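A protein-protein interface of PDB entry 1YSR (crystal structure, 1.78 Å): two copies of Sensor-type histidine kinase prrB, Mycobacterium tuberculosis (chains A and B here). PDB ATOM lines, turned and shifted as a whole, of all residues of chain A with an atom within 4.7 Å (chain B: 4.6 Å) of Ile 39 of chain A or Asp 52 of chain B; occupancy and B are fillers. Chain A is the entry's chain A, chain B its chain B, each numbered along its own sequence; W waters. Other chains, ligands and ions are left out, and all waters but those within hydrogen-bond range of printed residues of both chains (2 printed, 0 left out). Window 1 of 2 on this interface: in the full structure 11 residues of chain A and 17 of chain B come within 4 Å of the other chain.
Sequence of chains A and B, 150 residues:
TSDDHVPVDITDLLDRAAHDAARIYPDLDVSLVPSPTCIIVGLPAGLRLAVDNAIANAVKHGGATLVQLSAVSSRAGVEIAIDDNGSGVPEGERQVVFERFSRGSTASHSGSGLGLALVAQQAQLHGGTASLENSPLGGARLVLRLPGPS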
ATOM      1  N   PRO A   7     -35.973  12.943 -10.761  1.00  0.00           N
ATOM      2  CA  PRO A   7     -34.673  13.586 -10.641  1.00  0.00           C
ATOM      3  C   PRO A   7     -34.874  15.088 -10.585  1.00  0.00           C
ATOM      4  O   PRO A   7     -35.653  15.622 -11.359  1.00  0.00           O
ATOM      5  CB  PRO A   7     -33.966  13.173 -11.962  1.00  0.00           C
ATOM      6  CG  PRO A   7     -34.574  11.832 -12.289  1.00  0.00           C
ATOM      7  CD  PRO A   7     -36.049  12.157 -12.016  1.00  0.00           C
ATOM      8  N   VAL A   8     -34.204  15.757  -9.657  1.00  0.00           N
ATOM      9  CA  VAL A   8     -34.251  17.211  -9.542  1.00  0.00           C
ATOM     10  C   VAL A   8     -32.849  17.747  -9.421  1.00  0.00           C
ATOM     11  O   VAL A   8     -32.138  17.399  -8.527  1.00  0.00           O
ATOM     12  CB  VAL A   8     -35.023  17.666  -8.277  1.00  0.00           C
ATOM     13  CG1 VAL A   8     -35.162  19.150  -8.346  1.00  0.00           C
ATOM     14  CG2 VAL A   8     -36.431  17.066  -8.238  1.00  0.00           C
ATOM     15  N   ASP A   9     -32.461  18.634 -10.333  1.00  0.00           N
ATOM     16  CA  ASP A   9     -31.176  19.330 -10.190  1.00  0.00           C
ATOM     17  C   ASP A   9     -31.398  20.480  -9.234  1.00  0.00           C
ATOM     18  O   ASP A   9     -31.967  21.484  -9.630  1.00  0.00           O
ATOM     19  CB  ASP A   9     -30.716  19.860 -11.556  1.00  0.00           C
ATOM     20  CG  ASP A   9     -29.381  20.619 -11.479  1.00  0.00           C
ATOM     21  OD1 ASP A   9     -28.990  21.125 -10.395  1.00  0.00           O
ATOM     22  OD2 ASP A   9     -28.766  20.782 -12.550  1.00  0.00           O
ATOM     23  N   THR A  37     -23.123  21.076  -8.939  1.00  0.00           N
ATOM     24  CA  THR A  37     -24.406  20.519  -9.341  1.00  0.00           C
ATOM     25  C   THR A  37     -24.803  19.349  -8.481  1.00  0.00           C
ATOM     26  O   THR A  37     -24.030  18.376  -8.334  1.00  0.00           O
ATOM     27  CB  THR A  37     -24.413  20.151 -10.848  1.00  0.00           C
ATOM     28  OG1 THR A  37     -24.391  21.353 -11.606  1.00  0.00           O
ATOM     29  CG2 THR A  37     -25.663  19.411 -11.205  1.00  0.00           C
ATOM     30  N   CYS A  38     -25.985  19.448  -7.857  1.00  0.00           N
ATOM     31  CA  CYS A  38     -26.487  18.361  -7.041  1.00  0.00           C
ATOM     32  C   CYS A  38     -27.801  17.831  -7.539  1.00  0.00           C
ATOM     33  O   CYS A  38     -28.792  18.554  -7.579  1.00  0.00           O
ATOM     34  CB  CYS A  38     -26.643  18.742  -5.571  1.00  0.00           C
ATOM     35  SG  CYS A  38     -27.312  17.363  -4.590  1.00  0.00           S
ATOM     36  N   ILE A  39     -27.843  16.538  -7.855  1.00  0.00           N
ATOM     37  CA  ILE A  39     -29.118  15.941  -8.253  1.00  0.00           C
ATOM     38  C   ILE A  39     -29.670  15.117  -7.098  1.00  0.00           C
ATOM     39  O   ILE A  39     -28.915  14.290  -6.534  1.00  0.00           O
ATOM     40  CB  ILE A  39     -28.977  15.006  -9.496  1.00  0.00           C
ATOM     41  CG1 ILE A  39     -28.099  15.662 -10.604  1.00  0.00           C
ATOM     42  CG2 ILE A  39     -30.366  14.640 -10.032  1.00  0.00           C
ATOM     43  CD1 ILE A  39     -28.716  16.943 -11.166  1.00  0.00           C
ATOM     44  N   ILE A  40     -30.966  15.294  -6.771  1.00  0.00           N
ATOM     45  CA  ILE A  40     -31.643  14.388  -5.827  1.00  0.00           C
ATOM     46  C   ILE A  40     -32.881  13.874  -6.499  1.00  0.00           C
ATOM     47  O   ILE A  40     -33.175  14.245  -7.673  1.00  0.00           O
ATOM     48  CB  ILE A  40     -31.924  15.051  -4.417  1.00  0.00           C
ATOM     49  CG1 ILE A  40     -33.088  16.077  -4.530  1.00  0.00           C
ATOM     50  CG2 ILE A  40     -30.582  15.664  -3.811  1.00  0.00           C
ATOM     51  CD1 ILE A  40     -33.687  16.503  -3.179  1.00  0.00           C
ATOM     52  N   VAL A  41     -33.570  12.954  -5.841  1.00  0.00           N
ATOM     53  CA  VAL A  41     -34.847  12.532  -6.317  1.00  0.00           C
ATOM     54  C   VAL A  41     -35.850  13.157  -5.372  1.00  0.00           C
ATOM     55  O   VAL A  41     -35.687  13.093  -4.136  1.00  0.00           O
ATOM     56  CB  VAL A  41     -34.932  10.983  -6.325  1.00  0.00           C
ATOM     57  CG1 VAL A  41     -36.367  10.508  -6.514  1.00  0.00           C
ATOM     58  CG2 VAL A  41     -34.014  10.447  -7.484  1.00  0.00           C
ATOM     59  N   PRO A 149     -29.865  10.284  -3.338  1.00  0.00           N
ATOM     60  CA  PRO A 149     -30.490   9.144  -4.016  1.00  0.00           C
ATOM     61  C   PRO A 149     -29.655   7.867  -4.159  1.00  0.00           C
ATOM     62  O   PRO A 149     -30.201   6.832  -4.611  1.00  0.00           O
ATOM     63  CB  PRO A 149     -30.809   9.725  -5.403  1.00  0.00           C
ATOM     64  CG  PRO A 149     -29.648  10.668  -5.652  1.00  0.00           C
ATOM     65  CD  PRO A 149     -29.273  11.247  -4.309  1.00  0.00           C
ATOM     66  N   SER A 150     -28.373   7.958  -3.800  1.00  0.00           N
ATOM     67  CA  SER A 150     -27.397   6.858  -3.891  1.00  0.00           C
ATOM     68  C   SER A 150     -26.998   6.248  -2.540  1.00  0.00           C
ATOM     69  O   SER A 150     -27.063   6.907  -1.486  1.00  0.00           O
ATOM     70  CB  SER A 150     -26.131   7.367  -4.597  1.00  0.00           C
ATOM     71  OG  SER A 150     -26.474   7.863  -5.882  1.00  0.00           O
ATOM     72  OXT SER A 150     -26.564   5.074  -2.491  1.00  0.00           O
ATOM     73  N   ALA B  45     -31.005  16.211 -15.773  1.00  0.00           N
ATOM     74  CA  ALA B  45     -30.961  15.810 -14.344  1.00  0.00           C
ATOM     75  C   ALA B  45     -30.848  14.303 -14.211  1.00  0.00           C
ATOM     76  O   ALA B  45     -30.019  13.785 -13.441  1.00  0.00           O
ATOM     77  CB  ALA B  45     -32.193  16.327 -13.567  1.00  0.00           C
ATOM     78  N   ARG B  48     -27.431  12.997 -15.427  1.00  0.00           N
ATOM     79  CA  ARG B  48     -26.455  13.247 -14.373  1.00  0.00           C
ATOM     80  C   ARG B  48     -26.679  12.341 -13.174  1.00  0.00           C
ATOM     81  O   ARG B  48     -25.740  11.861 -12.550  1.00  0.00           O
ATOM     82  CB  ARG B  48     -26.465  14.735 -13.966  1.00  0.00           C
ATOM     83  CG  ARG B  48     -25.549  15.097 -12.824  1.00  0.00           C
ATOM     84  CD  ARG B  48     -24.057  14.910 -13.173  1.00  0.00           C
ATOM     85  NE  ARG B  48     -23.374  15.069 -11.877  1.00  0.00           N
ATOM     86  CZ  ARG B  48     -22.824  16.200 -11.441  1.00  0.00           C
ATOM     87  NH1 ARG B  48     -22.317  16.245 -10.216  1.00  0.00           N
ATOM     88  NH2 ARG B  48     -22.740  17.253 -12.236  1.00  0.00           N
ATOM     89  N   LEU B  49     -27.936  12.129 -12.822  1.00  0.00           N
ATOM     90  CA  LEU B  49     -28.227  11.227 -11.718  1.00  0.00           C
ATOM     91  C   LEU B  49     -27.631   9.855 -11.973  1.00  0.00           C
ATOM     92  O   LEU B  49     -27.004   9.245 -11.075  1.00  0.00           O
ATOM     93  CB  LEU B  49     -29.746  11.087 -11.600  1.00  0.00           C
ATOM     94  CG  LEU B  49     -30.220  10.154 -10.470  1.00  0.00           C
ATOM     95  CD1 LEU B  49     -29.617  10.506  -9.063  1.00  0.00           C
ATOM     96  CD2 LEU B  49     -31.744  10.065 -10.430  1.00  0.00           C
ATOM     97  N   ALA B  50     -27.838   9.355 -13.185  1.00  0.00           N
ATOM     98  CA  ALA B  50     -27.372   8.010 -13.557  1.00  0.00           C
ATOM     99  C   ALA B  50     -25.858   7.901 -13.370  1.00  0.00           C
ATOM    100  O   ALA B  50     -25.366   6.967 -12.728  1.00  0.00           O
ATOM    101  CB  ALA B  50     -27.748   7.727 -14.975  1.00  0.00           C
ATOM    102  N   VAL B  51     -25.124   8.875 -13.902  1.00  0.00           N
ATOM    103  CA  VAL B  51     -23.670   8.936 -13.692  1.00  0.00           C
ATOM    104  C   VAL B  51     -23.303   9.056 -12.234  1.00  0.00           C
ATOM    105  O   VAL B  51     -22.410   8.333 -11.758  1.00  0.00           O
ATOM    106  CB  VAL B  51     -23.050  10.109 -14.536  1.00  0.00           C
ATOM    107  CG1 VAL B  51     -21.530  10.188 -14.365  1.00  0.00           C
ATOM    108  CG2 VAL B  51     -23.341   9.897 -16.026  1.00  0.00           C
ATOM    109  N   ASP B  52     -23.988   9.957 -11.505  1.00  0.00           N
ATOM    110  CA  ASP B  52     -23.698  10.112 -10.083  1.00  0.00           C
ATOM    111  C   ASP B  52     -23.922   8.787  -9.400  1.00  0.00           C
ATOM    112  O   ASP B  52     -23.140   8.348  -8.559  1.00  0.00           O
ATOM    113  CB  ASP B  52     -24.642  11.105  -9.394  1.00  0.00           C
ATOM    114  CG  ASP B  52     -24.429  12.503  -9.791  1.00  0.00           C
ATOM    115  OD1 ASP B  52     -23.365  12.823 -10.355  1.00  0.00           O
ATOM    116  OD2 ASP B  52     -25.376  13.309  -9.522  1.00  0.00           O
ATOM    117  N   ASN B  53     -25.007   8.126  -9.757  1.00  0.00           N
ATOM    118  CA  ASN B  53     -25.341   6.910  -9.042  1.00  0.00           C
ATOM    119  C   ASN B  53     -24.321   5.815  -9.375  1.00  0.00           C
ATOM    120  O   ASN B  53     -23.942   5.024  -8.505  1.00  0.00           O
ATOM    121  CB  ASN B  53     -26.761   6.490  -9.360  1.00  0.00           C
ATOM    122  CG  ASN B  53     -27.195   5.251  -8.593  1.00  0.00           C
ATOM    123  OD1 ASN B  53     -27.566   4.244  -9.208  1.00  0.00           O
ATOM    124  ND2 ASN B  53     -27.212   5.341  -7.261  1.00  0.00           N
ATOM    125  N   ALA B  54     -23.840   5.820 -10.619  1.00  0.00           N
ATOM    126  CA  ALA B  54     -22.836   4.828 -11.019  1.00  0.00           C
ATOM    127  C   ALA B  54     -21.554   5.038 -10.225  1.00  0.00           C
ATOM    128  O   ALA B  54     -20.977   4.063  -9.741  1.00  0.00           O
ATOM    129  CB  ALA B  54     -22.578   4.893 -12.508  1.00  0.00           C
ATOM    130  N   ILE B  55     -21.123   6.299 -10.100  1.00  0.00           N
ATOM    131  CA  ILE B  55     -19.863   6.609  -9.434  1.00  0.00           C
ATOM    132  C   ILE B  55     -20.056   6.249  -7.967  1.00  0.00           C
ATOM    133  O   ILE B  55     -19.189   5.656  -7.323  1.00  0.00           O
ATOM    134  CB  ILE B  55     -19.493   8.101  -9.592  1.00  0.00           C
ATOM    135  CG1 ILE B  55     -19.184   8.437 -11.051  1.00  0.00           C
ATOM    136  CG2 ILE B  55     -18.293   8.429  -8.702  1.00  0.00           C
ATOM    137  CD1 ILE B  55     -19.290   9.905 -11.444  1.00  0.00           C
ATOM    138  N   ALA B  56     -21.238   6.576  -7.422  1.00  0.00           N
ATOM    139  CA  ALA B  56     -21.481   6.319  -6.004  1.00  0.00           C
ATOM    140  C   ALA B  56     -21.411   4.817  -5.693  1.00  0.00           C
ATOM    141  O   ALA B  56     -20.823   4.405  -4.696  1.00  0.00           O
ATOM    142  CB  ALA B  56     -22.822   6.898  -5.588  1.00  0.00           C
HETATM  143  O   HOH W   1     -25.066  15.474  -8.125  1.00  0.00           O
HETATM  144  O   HOH W   2     -26.789  12.495  -7.246  1.00  0.00           O
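Of the printed residues of chain B, Pro 7 of chain A touches Ala 45 and Leu 49.
Ile 39 of chain A touches just these residues of chain B: Ala 45 (3.5 Å), Arg 48 (3.4 Å), Leu 49 (3.9 Å) and Asp 52 (3.8 Å).
Of the printed residues of chain A, Asn 53 of chain B touches Ser 150 (3.0 Å).
The nearest printed residue of chain B that does not touch Ile 39 of chain A is Ala 50 of chain B (6.7 Å).
The nearest printed residue of chain A that does not touch Asn 53 of chain B is Pro 149 of chain A (4.3 Å).
The guanidinium group of Arg 48 of chain B lies within salt-bridge range of the side-chain carboxylate of Asp 52 of chain B, at 2.7 Å.
The side-chain hydroxyl (OG) of Ser 150 of chain A lies within hydrogen-bond range of the side-chain amide nitrogen (ND2) of Asn 53 of chain B (3.0 Å).
The backbone carbonyl oxygen of Thr 37 of chain A sits at hydrogen-bond distance from the guanidinium group of Arg 48 of chain B (3.3 Å).
Pro 7 of chain A touches Ala 45 of chain B (CB to CB, 3.96 Å).
Pro 7 of chain A touches Leu 49 of chain B (CG to CD2, 3.8 Å).
N of Asp 9 of chain A touches CB of Ala 45 of chain B, at 3.98 Å.
Ala 45 of chain B touches Ile 39 of chain A.
CG1 of Ile 39 of chain A touches CG of Arg 48 of chain B, 3.4 Å away.
Ile 39 of chain A touches Leu 49 of chain B.
Asp 52 of chain B touches Ile 39 of chain A.
CD2 of Leu 49 of chain B touches CG2 of Val 41 of chain A (3.7 Å).
Pro 149 of chain A touches Leu 49 of chain B (CG to CD1, 3.4 Å).
Ala 56 of chain B touches Ser 150 of chain A.
Water W1 lies within hydrogen-bond range of the side-chain carboxylate of Asp 52 of chain B (2.6 Å), the backbone NH of Ile 39 of chain A (3.0 Å) and the backbone carbonyl oxygen of Thr 37 of chain A (3.1 Å).
Water W2 bridges the side-chain carboxylate of Asp 52 of chain B and the backbone carbonyl oxygen of Ile 39 of chain A.
Hydrophobic or aromatic side chains of chain A within 4 Å of the printed part of chain B: Pro 7, Ile 39, Val 41 and Pro 149.
No position is printed for both chains.
Of the 12 pairs that touch across the chains among the printed residues, none has its exchanged pair printed and touching as well.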
